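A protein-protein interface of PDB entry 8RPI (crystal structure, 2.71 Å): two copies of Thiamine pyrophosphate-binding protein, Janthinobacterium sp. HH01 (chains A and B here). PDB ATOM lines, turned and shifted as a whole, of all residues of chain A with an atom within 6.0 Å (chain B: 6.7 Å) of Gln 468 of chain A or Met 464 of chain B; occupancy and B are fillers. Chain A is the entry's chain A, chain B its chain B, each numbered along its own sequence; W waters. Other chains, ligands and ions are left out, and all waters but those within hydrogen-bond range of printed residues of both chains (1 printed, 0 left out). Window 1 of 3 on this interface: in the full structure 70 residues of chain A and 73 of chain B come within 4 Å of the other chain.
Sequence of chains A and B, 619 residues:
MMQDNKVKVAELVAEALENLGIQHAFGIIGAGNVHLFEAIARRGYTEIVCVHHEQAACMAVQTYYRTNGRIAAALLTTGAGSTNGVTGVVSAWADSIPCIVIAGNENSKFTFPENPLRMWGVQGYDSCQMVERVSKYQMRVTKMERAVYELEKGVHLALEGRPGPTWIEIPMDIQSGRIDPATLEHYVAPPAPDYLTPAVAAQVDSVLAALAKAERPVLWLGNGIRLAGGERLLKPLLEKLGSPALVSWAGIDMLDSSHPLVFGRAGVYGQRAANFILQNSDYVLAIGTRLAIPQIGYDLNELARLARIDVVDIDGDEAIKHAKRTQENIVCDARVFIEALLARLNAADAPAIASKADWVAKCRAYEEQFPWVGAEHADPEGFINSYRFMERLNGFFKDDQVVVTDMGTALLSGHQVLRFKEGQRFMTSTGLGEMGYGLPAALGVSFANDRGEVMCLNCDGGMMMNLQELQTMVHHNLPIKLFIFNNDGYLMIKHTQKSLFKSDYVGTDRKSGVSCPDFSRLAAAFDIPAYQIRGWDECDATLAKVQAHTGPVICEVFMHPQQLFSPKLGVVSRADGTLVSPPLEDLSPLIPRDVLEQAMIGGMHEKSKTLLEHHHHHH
Among the printed residues, merely in contact across the chains: His 52 of chain A with Met 464 of chain B, His 53 of chain A with Met 465 of chain B, Met 464 of chain A with Gln 468 of chain B, Met 465 of chain A with His 53 of chain B, Met 465 of chain A with Gln 468 of chain B, Gln 468 of chain A with Met 464 of chain B, Gln 471 of chain A with Met 464 of chain B, Gln 471 of chain A with Cys 516 of chain B, Phe 526 of chain A with Pro 517 of chain B and Phe 526 of chain A with Leu 522 of chain B.
His 53 of chain A touches Met 465 of chain B, and with the chains exchanged Met 465 of chain A touches His 53 of chain B.
Met 464 of chain A touches Gln 468 of chain B, and with the chains exchanged Gln 468 of chain A touches Met 464 of chain B.
Met 465 of chain A touches Gln 468 of chain B, but with the chains exchanged Gln 468 of chain A does not touch Met 465 of chain B (4.4 Å).
Positions printed for both chains: 53, 463, 464, 465, 466, 467 and 468.
Water W1 lies within hydrogen-bond range of OD1 of Asn 466 of chain A (2.6 Å), NE2 of His 53 of chain B (3.0 Å) and ND1 of His 53 of chain A (3.1 Å).
Hydrophobic or aromatic side chains of chain B within 4 Å of the printed part of chain A: His 53, Met 464, Met 465, Pro 517 and Leu 522.
Printed residues of chain A that touch a printed residue of chain B: His 52, His 53, Met 464, Met 465, Gln 468, Gln 471 and Phe 526.
Hydrophobic or aromatic side chains of chain A that line the printed part of chain B: His 52, His 53, Met 464 and Phe 526.
Among the printed residues, no Asp or Glu carboxylate lies within 4 Å of a Lys or Arg side-chain nitrogen of the other chain.
The backbone carbonyl oxygen of His 52 of chain A sits close to the side-chain sulfur of Met 465 of chain B.
NE2 of Gln 471 of chain A lies within hydrogen-bond range of OG of Ser 515 of chain B (2.8 Å).
The backbone carbonyl oxygen (O) of Ser 515 of chain B sits close to a ring nitrogen (NE2) of His 52 of chain A (3.0 Å).
The side-chain amide oxygen (OE1) of Gln 471 of chain A lies close to the backbone nitrogen (N) of Pro 517 of chain B (3.3 Å).
Leu 467 of chain A touches none of the printed residues of chain B.
Of the printed residues of chain A, His 53 of chain B touches Met 465.
Cys 459 of chain B touches none of the printed residues of chain A.
Met 464 of chain B touches just these residues of chain A: His 52 (3.4 Å), Gln 468 (3.1 Å) and Gln 471 (3.9 Å).
Of the printed residues of chain A, Leu 522 of chain B touches Phe 526 (3.6 Å).
The nearest residue of chain B that does not touch Gln 468 of chain A is Gln 468 of chain B (4.2 Å).
The nearest residue of chain A that does not touch Met 464 of chain B is Phe 526 of chain A (5.1 Å).
The nearest printed residue of chain A that does not touch Leu 522 of chain B is Gln 471 of chain A (6.8 Å).
OD1 of Asn 466 of chain A sits at hydrogen-bond distance from NE2 of Gln 468 of chain A, 3.2 Å away.
The backbone carbonyl oxygen of Asp 460 of chain B sits at hydrogen-bond distance from the side-chain sulfur of Cys 516 of chain B, 3.5 Å away.
The backbone NH (N) of His 52 of chain A sits at hydrogen-bond distance from the side-chain carboxylate (OE2) of Glu 469 of chain A (3.1 Å).
The backbone NH of His 53 of chain A is in hydrogen-bond range of the side-chain carboxylate of Glu 469 of chain A (3.4 Å).
The side-chain amide oxygen (OD1) of Asn 466 of chain B lies within hydrogen-bond range of the side-chain amide nitrogen (NE2) of Gln 468 of chain B, 2.9 Å away.
The side-chain amide nitrogen (NE2) of Gln 468 of chain A is in hydrogen-bond range of the side-chain carboxylate (OE2) of Glu 469 of chain A.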
ATOM      1  N   HIS A  52      14.957  -2.952 -11.831  1.00  0.00           N
ATOM      2  CA  HIS A  52      14.921  -4.403 -11.692  1.00  0.00           C
ATOM      3  C   HIS A  52      13.796  -5.044 -12.497  1.00  0.00           C
ATOM      4  O   HIS A  52      13.509  -6.233 -12.313  1.00  0.00           O
ATOM      5  CB  HIS A  52      14.803  -4.787 -10.217  1.00  0.00           C
ATOM      6  CG  HIS A  52      16.049  -4.524  -9.429  1.00  0.00           C
ATOM      7  ND1 HIS A  52      17.127  -5.383  -9.438  1.00  0.00           N
ATOM      8  CD2 HIS A  52      16.391  -3.498  -8.615  1.00  0.00           C
ATOM      9  CE1 HIS A  52      18.078  -4.899  -8.658  1.00  0.00           C
ATOM     10  NE2 HIS A  52      17.657  -3.755  -8.147  1.00  0.00           N
ATOM     11  N   HIS A  53      13.149  -4.282 -13.377  1.00  0.00           N
ATOM     12  CA  HIS A  53      12.232  -4.836 -14.365  1.00  0.00           C
ATOM     13  C   HIS A  53      12.006  -3.763 -15.420  1.00  0.00           C
ATOM     14  O   HIS A  53      11.625  -2.640 -15.083  1.00  0.00           O
ATOM     15  CB  HIS A  53      10.916  -5.259 -13.724  1.00  0.00           C
ATOM     16  CG  HIS A  53      10.056  -6.115 -14.604  1.00  0.00           C
ATOM     17  ND1 HIS A  53       9.519  -5.664 -15.791  1.00  0.00           N
ATOM     18  CD2 HIS A  53       9.619  -7.387 -14.454  1.00  0.00           C
ATOM     19  CE1 HIS A  53       8.801  -6.627 -16.340  1.00  0.00           C
ATOM     20  NE2 HIS A  53       8.845  -7.683 -15.549  1.00  0.00           N
ATOM     21  N   ALA A  56       9.315  -1.066 -15.288  1.00  0.00           N
ATOM     22  CA  ALA A  56       9.467   0.142 -14.487  1.00  0.00           C
ATOM     23  C   ALA A  56      10.220   1.226 -15.242  1.00  0.00           C
ATOM     24  O   ALA A  56       9.990   2.420 -15.010  1.00  0.00           O
ATOM     25  CB  ALA A  56      10.192  -0.186 -13.184  1.00  0.00           C
ATOM     26  N   LEU A 439       5.098   2.921  -7.885  1.00  0.00           N
ATOM     27  CA  LEU A 439       6.527   2.994  -7.581  1.00  0.00           C
ATOM     28  C   LEU A 439       7.325   3.517  -8.766  1.00  0.00           C
ATOM     29  O   LEU A 439       8.053   4.513  -8.609  1.00  0.00           O
ATOM     30  CB  LEU A 439       7.045   1.627  -7.119  1.00  0.00           C
ATOM     31  CG  LEU A 439       6.503   1.077  -5.799  1.00  0.00           C
ATOM     32  CD1 LEU A 439       7.110  -0.288  -5.510  1.00  0.00           C
ATOM     33  CD2 LEU A 439       6.774   2.029  -4.642  1.00  0.00           C
ATOM     34  N   MET A 463       1.007  -2.930  -5.394  1.00  0.00           N
ATOM     35  CA  MET A 463       2.390  -2.929  -4.933  1.00  0.00           C
ATOM     36  C   MET A 463       3.158  -4.143  -5.438  1.00  0.00           C
ATOM     37  O   MET A 463       4.383  -4.079  -5.597  1.00  0.00           O
ATOM     38  CB  MET A 463       2.426  -2.892  -3.405  1.00  0.00           C
ATOM     39  CG  MET A 463       2.450  -1.490  -2.815  1.00  0.00           C
ATOM     40  SD  MET A 463       3.992  -0.613  -3.135  1.00  0.00           S
ATOM     41  CE  MET A 463       5.159  -1.713  -2.340  1.00  0.00           C
ATOM     42  N   MET A 464       2.459  -5.250  -5.697  1.00  0.00           N
ATOM     43  CA  MET A 464       3.120  -6.501  -6.045  1.00  0.00           C
ATOM     44  C   MET A 464       3.651  -6.505  -7.473  1.00  0.00           C
ATOM     45  O   MET A 464       4.680  -7.134  -7.737  1.00  0.00           O
ATOM     46  CB  MET A 464       2.150  -7.672  -5.849  1.00  0.00           C
ATOM     47  CG  MET A 464       1.519  -7.727  -4.462  1.00  0.00           C
ATOM     48  SD  MET A 464       2.739  -7.932  -3.152  1.00  0.00           S
ATOM     49  CE  MET A 464       3.295  -9.604  -3.464  1.00  0.00           C
ATOM     50  N   MET A 465       2.979  -5.820  -8.401  1.00  0.00           N
ATOM     51  CA  MET A 465       3.387  -5.888  -9.802  1.00  0.00           C
ATOM     52  C   MET A 465       4.854  -5.508  -9.970  1.00  0.00           C
ATOM     53  O   MET A 465       5.622  -6.226 -10.621  1.00  0.00           O
ATOM     54  CB  MET A 465       2.491  -4.986 -10.653  1.00  0.00           C
ATOM     55  CG  MET A 465       1.240  -5.681 -11.185  1.00  0.00           C
ATOM     56  SD  MET A 465       0.208  -6.359  -9.866  1.00  0.00           S
ATOM     57  CE  MET A 465      -1.183  -7.012 -10.790  1.00  0.00           C
ATOM     58  N   ASN A 466       5.262  -4.386  -9.377  1.00  0.00           N
ATOM     59  CA  ASN A 466       6.630  -3.885  -9.455  1.00  0.00           C
ATOM     60  C   ASN A 466       7.244  -3.763  -8.063  1.00  0.00           C
ATOM     61  O   ASN A 466       7.951  -2.800  -7.749  1.00  0.00           O
ATOM     62  CB  ASN A 466       6.673  -2.544 -10.185  1.00  0.00           C
ATOM     63  CG  ASN A 466       6.407  -2.684 -11.671  1.00  0.00           C
ATOM     64  OD1 ASN A 466       6.943  -3.576 -12.333  1.00  0.00           O
ATOM     65  ND2 ASN A 466       5.569  -1.806 -12.203  1.00  0.00           N
ATOM     66  N   LEU A 467       6.967  -4.755  -7.214  1.00  0.00           N
ATOM     67  CA  LEU A 467       7.524  -4.772  -5.866  1.00  0.00           C
ATOM     68  C   LEU A 467       9.033  -4.568  -5.888  1.00  0.00           C
ATOM     69  O   LEU A 467       9.593  -3.900  -5.010  1.00  0.00           O
ATOM     70  CB  LEU A 467       7.173  -6.102  -5.196  1.00  0.00           C
ATOM     71  CG  LEU A 467       7.413  -6.283  -3.698  1.00  0.00           C
ATOM     72  CD1 LEU A 467       6.502  -5.363  -2.883  1.00  0.00           C
ATOM     73  CD2 LEU A 467       7.199  -7.743  -3.325  1.00  0.00           C
ATOM     74  N   GLN A 468       9.704  -5.125  -6.900  1.00  0.00           N
ATOM     75  CA  GLN A 468      11.161  -5.153  -6.935  1.00  0.00           C
ATOM     76  C   GLN A 468      11.781  -3.763  -6.955  1.00  0.00           C
ATOM     77  O   GLN A 468      12.976  -3.629  -6.672  1.00  0.00           O
ATOM     78  CB  GLN A 468      11.635  -5.943  -8.161  1.00  0.00           C
ATOM     79  CG  GLN A 468      11.425  -5.248  -9.508  1.00  0.00           C
ATOM     80  CD  GLN A 468       9.976  -5.204  -9.936  1.00  0.00           C
ATOM     81  OE1 GLN A 468       9.168  -6.024  -9.504  1.00  0.00           O
ATOM     82  NE2 GLN A 468       9.639  -4.244 -10.793  1.00  0.00           N
ATOM     83  N   GLU A 469      11.013  -2.735  -7.297  1.00  0.00           N
ATOM     84  CA  GLU A 469      11.558  -1.387  -7.361  1.00  0.00           C
ATOM     85  C   GLU A 469      11.753  -0.764  -5.986  1.00  0.00           C
ATOM     86  O   GLU A 469      12.258   0.361  -5.900  1.00  0.00           O
ATOM     87  CB  GLU A 469      10.653  -0.502  -8.219  1.00  0.00           C
ATOM     88  CG  GLU A 469      10.547  -0.973  -9.665  1.00  0.00           C
ATOM     89  CD  GLU A 469      11.903  -1.141 -10.314  1.00  0.00           C
ATOM     90  OE1 GLU A 469      12.759  -0.248 -10.146  1.00  0.00           O
ATOM     91  OE2 GLU A 469      12.122  -2.177 -10.972  1.00  0.00           O
ATOM     92  N   LEU A 470      11.371  -1.457  -4.912  1.00  0.00           N
ATOM     93  CA  LEU A 470      11.781  -1.012  -3.586  1.00  0.00           C
ATOM     94  C   LEU A 470      13.299  -1.028  -3.459  1.00  0.00           C
ATOM     95  O   LEU A 470      13.879  -0.158  -2.798  1.00  0.00           O
ATOM     96  CB  LEU A 470      11.136  -1.891  -2.515  1.00  0.00           C
ATOM     97  CG  LEU A 470       9.616  -1.738  -2.370  1.00  0.00           C
ATOM     98  CD1 LEU A 470       9.084  -2.716  -1.331  1.00  0.00           C
ATOM     99  CD2 LEU A 470       9.222  -0.305  -2.016  1.00  0.00           C
ATOM    100  N   GLN A 471      13.957  -1.997  -4.102  1.00  0.00           N
ATOM    101  CA  GLN A 471      15.414  -2.067  -4.063  1.00  0.00           C
ATOM    102  C   GLN A 471      16.042  -0.897  -4.806  1.00  0.00           C
ATOM    103  O   GLN A 471      17.073  -0.363  -4.381  1.00  0.00           O
ATOM    104  CB  GLN A 471      15.890  -3.392  -4.660  1.00  0.00           C
ATOM    105  CG  GLN A 471      17.403  -3.579  -4.638  1.00  0.00           C
ATOM    106  CD  GLN A 471      17.961  -3.640  -3.226  1.00  0.00           C
ATOM    107  OE1 GLN A 471      17.288  -4.092  -2.298  1.00  0.00           O
ATOM    108  NE2 GLN A 471      19.196  -3.180  -3.058  1.00  0.00           N
ATOM    109  N   THR A 472      15.448  -0.499  -5.933  1.00  0.00           N
ATOM    110  CA  THR A 472      15.894   0.710  -6.615  1.00  0.00           C
ATOM    111  C   THR A 472      15.735   1.929  -5.716  1.00  0.00           C
ATOM    112  O   THR A 472      16.586   2.826  -5.714  1.00  0.00           O
ATOM    113  CB  THR A 472      15.100   0.896  -7.907  1.00  0.00           C
ATOM    114  OG1 THR A 472      15.105  -0.327  -8.654  1.00  0.00           O
ATOM    115  CG2 THR A 472      15.699   2.015  -8.745  1.00  0.00           C
ATOM    116  N   PHE A 526      14.108  -4.375   3.603  1.00  0.00           N
ATOM    117  CA  PHE A 526      14.739  -3.432   2.690  1.00  0.00           C
ATOM    118  C   PHE A 526      15.399  -2.252   3.403  1.00  0.00           C
ATOM    119  O   PHE A 526      15.844  -1.313   2.733  1.00  0.00           O
ATOM    120  CB  PHE A 526      13.708  -2.891   1.694  1.00  0.00           C
ATOM    121  CG  PHE A 526      13.347  -3.852   0.599  1.00  0.00           C
ATOM    122  CD1 PHE A 526      14.253  -4.147  -0.402  1.00  0.00           C
ATOM    123  CD2 PHE A 526      12.094  -4.437   0.556  1.00  0.00           C
ATOM    124  CE1 PHE A 526      13.924  -5.021  -1.413  1.00  0.00           C
ATOM    125  CE2 PHE A 526      11.759  -5.310  -0.454  1.00  0.00           C
ATOM    126  CZ  PHE A 526      12.672  -5.604  -1.440  1.00  0.00           C
ATOM    127  N   HIS B  53       1.824 -11.099 -10.986  1.00  0.00           N
ATOM    128  CA  HIS B  53       2.161 -10.449 -12.246  1.00  0.00           C
ATOM    129  C   HIS B  53       1.797 -11.415 -13.363  1.00  0.00           C
ATOM    130  O   HIS B  53       2.187 -12.585 -13.318  1.00  0.00           O
ATOM    131  CB  HIS B  53       3.645 -10.075 -12.300  1.00  0.00           C
ATOM    132  CG  HIS B  53       3.985  -9.068 -13.358  1.00  0.00           C
ATOM    133  ND1 HIS B  53       4.112  -9.398 -14.690  1.00  0.00           N
ATOM    134  CD2 HIS B  53       4.247  -7.742 -13.274  1.00  0.00           C
ATOM    135  CE1 HIS B  53       4.426  -8.316 -15.383  1.00  0.00           C
ATOM    136  NE2 HIS B  53       4.515  -7.299 -14.546  1.00  0.00           N
ATOM    137  N   MET B 435      15.462 -13.371 -17.632  1.00  0.00           N
ATOM    138  CA  MET B 435      15.601 -13.384 -16.186  1.00  0.00           C
ATOM    139  C   MET B 435      14.225 -13.376 -15.541  1.00  0.00           C
ATOM    140  O   MET B 435      13.269 -12.801 -16.071  1.00  0.00           O
ATOM    141  CB  MET B 435      16.394 -12.176 -15.697  1.00  0.00           C
ATOM    142  CG  MET B 435      17.852 -12.175 -16.076  1.00  0.00           C
ATOM    143  SD  MET B 435      18.571 -10.565 -15.712  1.00  0.00           S
ATOM    144  CE  MET B 435      18.435 -10.519 -13.922  1.00  0.00           C
ATOM    145  N   GLY B 436      14.132 -14.014 -14.381  1.00  0.00           N
ATOM    146  CA  GLY B 436      12.879 -14.084 -13.666  1.00  0.00           C
ATOM    147  C   GLY B 436      12.002 -15.248 -14.050  1.00  0.00           C
ATOM    148  O   GLY B 436      10.796 -15.211 -13.777  1.00  0.00           O
ATOM    149  N   ASN B 458      18.270 -20.226  -8.468  1.00  0.00           N
ATOM    150  CA  ASN B 458      18.014 -18.852  -8.866  1.00  0.00           C
ATOM    151  C   ASN B 458      19.212 -17.984  -8.502  1.00  0.00           C
ATOM    152  O   ASN B 458      20.186 -18.448  -7.901  1.00  0.00           O
ATOM    153  CB  ASN B 458      16.726 -18.326  -8.215  1.00  0.00           C
ATOM    154  CG  ASN B 458      16.016 -17.306  -9.077  1.00  0.00           C
ATOM    155  OD1 ASN B 458      16.630 -16.359  -9.570  1.00  0.00           O
ATOM    156  ND2 ASN B 458      14.715 -17.498  -9.274  1.00  0.00           N
ATOM    157  N   CYS B 459      19.133 -16.710  -8.886  1.00  0.00           N
ATOM    158  CA  CYS B 459      20.230 -15.769  -8.735  1.00  0.00           C
ATOM    159  C   CYS B 459      19.718 -14.466  -8.137  1.00  0.00           C
ATOM    160  O   CYS B 459      18.527 -14.153  -8.202  1.00  0.00           O
ATOM    161  CB  CYS B 459      20.902 -15.477 -10.078  1.00  0.00           C
ATOM    162  SG  CYS B 459      21.190 -16.934 -11.092  1.00  0.00           S
ATOM    163  N   ASP B 460      20.646 -13.692  -7.572  1.00  0.00           N
ATOM    164  CA  ASP B 460      20.258 -12.451  -6.910  1.00  0.00           C
ATOM    165  C   ASP B 460      19.647 -11.461  -7.898  1.00  0.00           C
ATOM    166  O   ASP B 460      18.707 -10.734  -7.554  1.00  0.00           O
ATOM    167  CB  ASP B 460      21.462 -11.838  -6.193  1.00  0.00           C
ATOM    168  CG  ASP B 460      22.639 -11.596  -7.121  1.00  0.00           C
ATOM    169  OD1 ASP B 460      22.559 -11.992  -8.302  1.00  0.00           O
ATOM    170  OD2 ASP B 460      23.644 -11.009  -6.667  1.00  0.00           O
ATOM    171  N   GLY B 461      20.154 -11.420  -9.128  1.00  0.00           N
ATOM    172  CA  GLY B 461      19.593 -10.530 -10.128  1.00  0.00           C
ATOM    173  C   GLY B 461      18.269 -11.036 -10.670  1.00  0.00           C
ATOM    174  O   GLY B 461      17.317 -10.266 -10.825  1.00  0.00           O
ATOM    175  N   GLY B 462      18.194 -12.339 -10.952  1.00  0.00           N
ATOM    176  CA  GLY B 462      16.993 -12.892 -11.556  1.00  0.00           C
ATOM    177  C   GLY B 462      15.831 -12.992 -10.591  1.00  0.00           C
ATOM    178  O   GLY B 462      14.669 -12.971 -11.009  1.00  0.00           O
ATOM    179  N   MET B 463      16.123 -13.110  -9.295  1.00  0.00           N
ATOM    180  CA  MET B 463      15.075 -13.106  -8.284  1.00  0.00           C
ATOM    181  C   MET B 463      14.229 -11.841  -8.319  1.00  0.00           C
ATOM    182  O   MET B 463      13.103 -11.848  -7.810  1.00  0.00           O
ATOM    183  CB  MET B 463      15.694 -13.248  -6.893  1.00  0.00           C
ATOM    184  CG  MET B 463      15.952 -14.677  -6.462  1.00  0.00           C
ATOM    185  SD  MET B 463      14.430 -15.615  -6.268  1.00  0.00           S
ATOM    186  CE  MET B 463      13.564 -14.622  -5.049  1.00  0.00           C
ATOM    187  N   MET B 464      14.738 -10.758  -8.901  1.00  0.00           N
ATOM    188  CA  MET B 464      14.039  -9.484  -8.799  1.00  0.00           C
ATOM    189  C   MET B 464      12.913  -9.353  -9.817  1.00  0.00           C
ATOM    190  O   MET B 464      11.897  -8.716  -9.516  1.00  0.00           O
ATOM    191  CB  MET B 464      15.031  -8.328  -8.955  1.00  0.00           C
ATOM    192  CG  MET B 464      16.206  -8.366  -7.975  1.00  0.00           C
ATOM    193  SD  MET B 464      15.747  -8.365  -6.225  1.00  0.00           S
ATOM    194  CE  MET B 464      14.830  -6.834  -6.119  1.00  0.00           C
ATOM    195  N   MET B 465      13.056  -9.948 -11.007  1.00  0.00           N
ATOM    196  CA  MET B 465      12.068  -9.725 -12.061  1.00  0.00           C
ATOM    197  C   MET B 465      10.674 -10.181 -11.648  1.00  0.00           C
ATOM    198  O   MET B 465       9.678  -9.572 -12.058  1.00  0.00           O
ATOM    199  CB  MET B 465      12.485 -10.438 -13.349  1.00  0.00           C
ATOM    200  CG  MET B 465      13.315  -9.583 -14.295  1.00  0.00           C
ATOM    201  SD  MET B 465      14.900  -9.101 -13.584  1.00  0.00           S
ATOM    202  CE  MET B 465      15.720  -8.424 -15.026  1.00  0.00           C
ATOM    203  N   ASN B 466      10.573 -11.240 -10.848  1.00  0.00           N
ATOM    204  CA  ASN B 466       9.287 -11.747 -10.378  1.00  0.00           C
ATOM    205  C   ASN B 466       9.346 -12.047  -8.889  1.00  0.00           C
ATOM    206  O   ASN B 466       8.797 -13.043  -8.410  1.00  0.00           O
ATOM    207  CB  ASN B 466       8.863 -12.989 -11.159  1.00  0.00           C
ATOM    208  CG  ASN B 466       8.427 -12.664 -12.566  1.00  0.00           C
ATOM    209  OD1 ASN B 466       7.538 -11.838 -12.782  1.00  0.00           O
ATOM    210  ND2 ASN B 466       9.064 -13.303 -13.541  1.00  0.00           N
ATOM    211  N   LEU B 467      10.033 -11.181  -8.140  1.00  0.00           N
ATOM    212  CA  LEU B 467      10.085 -11.305  -6.689  1.00  0.00           C
ATOM    213  C   LEU B 467       8.697 -11.416  -6.075  1.00  0.00           C
ATOM    214  O   LEU B 467       8.525 -12.067  -5.039  1.00  0.00           O
ATOM    215  CB  LEU B 467      10.815 -10.097  -6.106  1.00  0.00           C
ATOM    216  CG  LEU B 467      11.077 -10.097  -4.603  1.00  0.00           C
ATOM    217  CD1 LEU B 467      12.110 -11.150  -4.251  1.00  0.00           C
ATOM    218  CD2 LEU B 467      11.528  -8.714  -4.170  1.00  0.00           C
ATOM    219  N   GLN B 468       7.695 -10.792  -6.695  1.00  0.00           N
ATOM    220  CA  GLN B 468       6.356 -10.790  -6.122  1.00  0.00           C
ATOM    221  C   GLN B 468       5.780 -12.192  -5.978  1.00  0.00           C
ATOM    222  O   GLN B 468       4.849 -12.387  -5.188  1.00  0.00           O
ATOM    223  CB  GLN B 468       5.418  -9.930  -6.976  1.00  0.00           C
ATOM    224  CG  GLN B 468       5.021 -10.538  -8.320  1.00  0.00           C
ATOM    225  CD  GLN B 468       6.113 -10.446  -9.365  1.00  0.00           C
ATOM    226  OE1 GLN B 468       6.992  -9.584  -9.291  1.00  0.00           O
ATOM    227  NE2 GLN B 468       6.058 -11.333 -10.353  1.00  0.00           N
ATOM    228  N   TYR B 490      25.119  -8.674 -11.653  1.00  0.00           N
ATOM    229  CA  TYR B 490      24.996  -9.409 -12.910  1.00  0.00           C
ATOM    230  C   TYR B 490      26.365  -9.963 -13.299  1.00  0.00           C
ATOM    231  O   TYR B 490      27.082  -9.408 -14.133  1.00  0.00           O
ATOM    232  CB  TYR B 490      24.429  -8.504 -13.996  1.00  0.00           C
ATOM    233  CG  TYR B 490      23.080  -7.887 -13.676  1.00  0.00           C
ATOM    234  CD1 TYR B 490      22.226  -8.464 -12.746  1.00  0.00           C
ATOM    235  CD2 TYR B 490      22.660  -6.730 -14.315  1.00  0.00           C
ATOM    236  CE1 TYR B 490      20.992  -7.901 -12.461  1.00  0.00           C
ATOM    237  CE2 TYR B 490      21.431  -6.160 -14.036  1.00  0.00           C
ATOM    238  CZ  TYR B 490      20.601  -6.748 -13.112  1.00  0.00           C
ATOM    239  OH  TYR B 490      19.378  -6.182 -12.839  1.00  0.00           O
ATOM    240  N   SER B 515      22.044  -3.187  -7.124  1.00  0.00           N
ATOM    241  CA  SER B 515      22.159  -3.871  -5.848  1.00  0.00           C
ATOM    242  C   SER B 515      20.959  -4.787  -5.662  1.00  0.00           C
ATOM    243  O   SER B 515      19.933  -4.647  -6.333  1.00  0.00           O
ATOM    244  CB  SER B 515      22.257  -2.881  -4.684  1.00  0.00           C
ATOM    245  OG  SER B 515      21.167  -1.981  -4.700  1.00  0.00           O
ATOM    246  N   CYS B 516      21.103  -5.733  -4.744  1.00  0.00           N
ATOM    247  CA  CYS B 516      20.060  -6.696  -4.441  1.00  0.00           C
ATOM    248  C   CYS B 516      19.895  -6.821  -2.934  1.00  0.00           C
ATOM    249  O   CYS B 516      20.864  -6.674  -2.185  1.00  0.00           O
ATOM    250  CB  CYS B 516      20.393  -8.065  -5.048  1.00  0.00           C
ATOM    251  SG  CYS B 516      20.721  -7.993  -6.829  1.00  0.00           S
ATOM    252  N   PRO B 517      18.682  -7.088  -2.464  1.00  0.00           N
ATOM    253  CA  PRO B 517      18.437  -7.147  -1.020  1.00  0.00           C
ATOM    254  C   PRO B 517      18.975  -8.430  -0.397  1.00  0.00           C
ATOM    255  O   PRO B 517      19.377  -9.375  -1.076  1.00  0.00           O
ATOM    256  CB  PRO B 517      16.909  -7.086  -0.925  1.00  0.00           C
ATOM    257  CG  PRO B 517      16.445  -7.712  -2.187  1.00  0.00           C
ATOM    258  CD  PRO B 517      17.452  -7.331  -3.240  1.00  0.00           C
ATOM    259  N   PHE B 519      18.218 -11.664   0.901  1.00  0.00           N
ATOM    260  CA  PHE B 519      17.069 -12.533   0.670  1.00  0.00           C
ATOM    261  C   PHE B 519      16.710 -13.374   1.891  1.00  0.00           C
ATOM    262  O   PHE B 519      15.575 -13.856   1.979  1.00  0.00           O
ATOM    263  CB  PHE B 519      17.330 -13.434  -0.538  1.00  0.00           C
ATOM    264  CG  PHE B 519      17.417 -12.686  -1.842  1.00  0.00           C
ATOM    265  CD1 PHE B 519      16.269 -12.260  -2.492  1.00  0.00           C
ATOM    266  CD2 PHE B 519      18.644 -12.407  -2.417  1.00  0.00           C
ATOM    267  CE1 PHE B 519      16.346 -11.570  -3.689  1.00  0.00           C
ATOM    268  CE2 PHE B 519      18.727 -11.719  -3.614  1.00  0.00           C
ATOM    269  CZ  PHE B 519      17.576 -11.300  -4.250  1.00  0.00           C
ATOM    270  N   LEU B 522      14.345 -10.881   3.590  1.00  0.00           N
ATOM    271  CA  LEU B 522      13.052 -10.928   2.918  1.00  0.00           C
ATOM    272  C   LEU B 522      12.316 -12.210   3.266  1.00  0.00           C
ATOM    273  O   LEU B 522      11.115 -12.189   3.551  1.00  0.00           O
ATOM    274  CB  LEU B 522      13.230 -10.833   1.404  1.00  0.00           C
ATOM    275  CG  LEU B 522      13.523  -9.467   0.787  1.00  0.00           C
ATOM    276  CD1 LEU B 522      13.698  -9.606  -0.720  1.00  0.00           C
ATOM    277  CD2 LEU B 522      12.414  -8.477   1.104  1.00  0.00           C
HETATM  278  O   HOH W   1       6.910  -5.509 -14.140  1.00  0.00           O
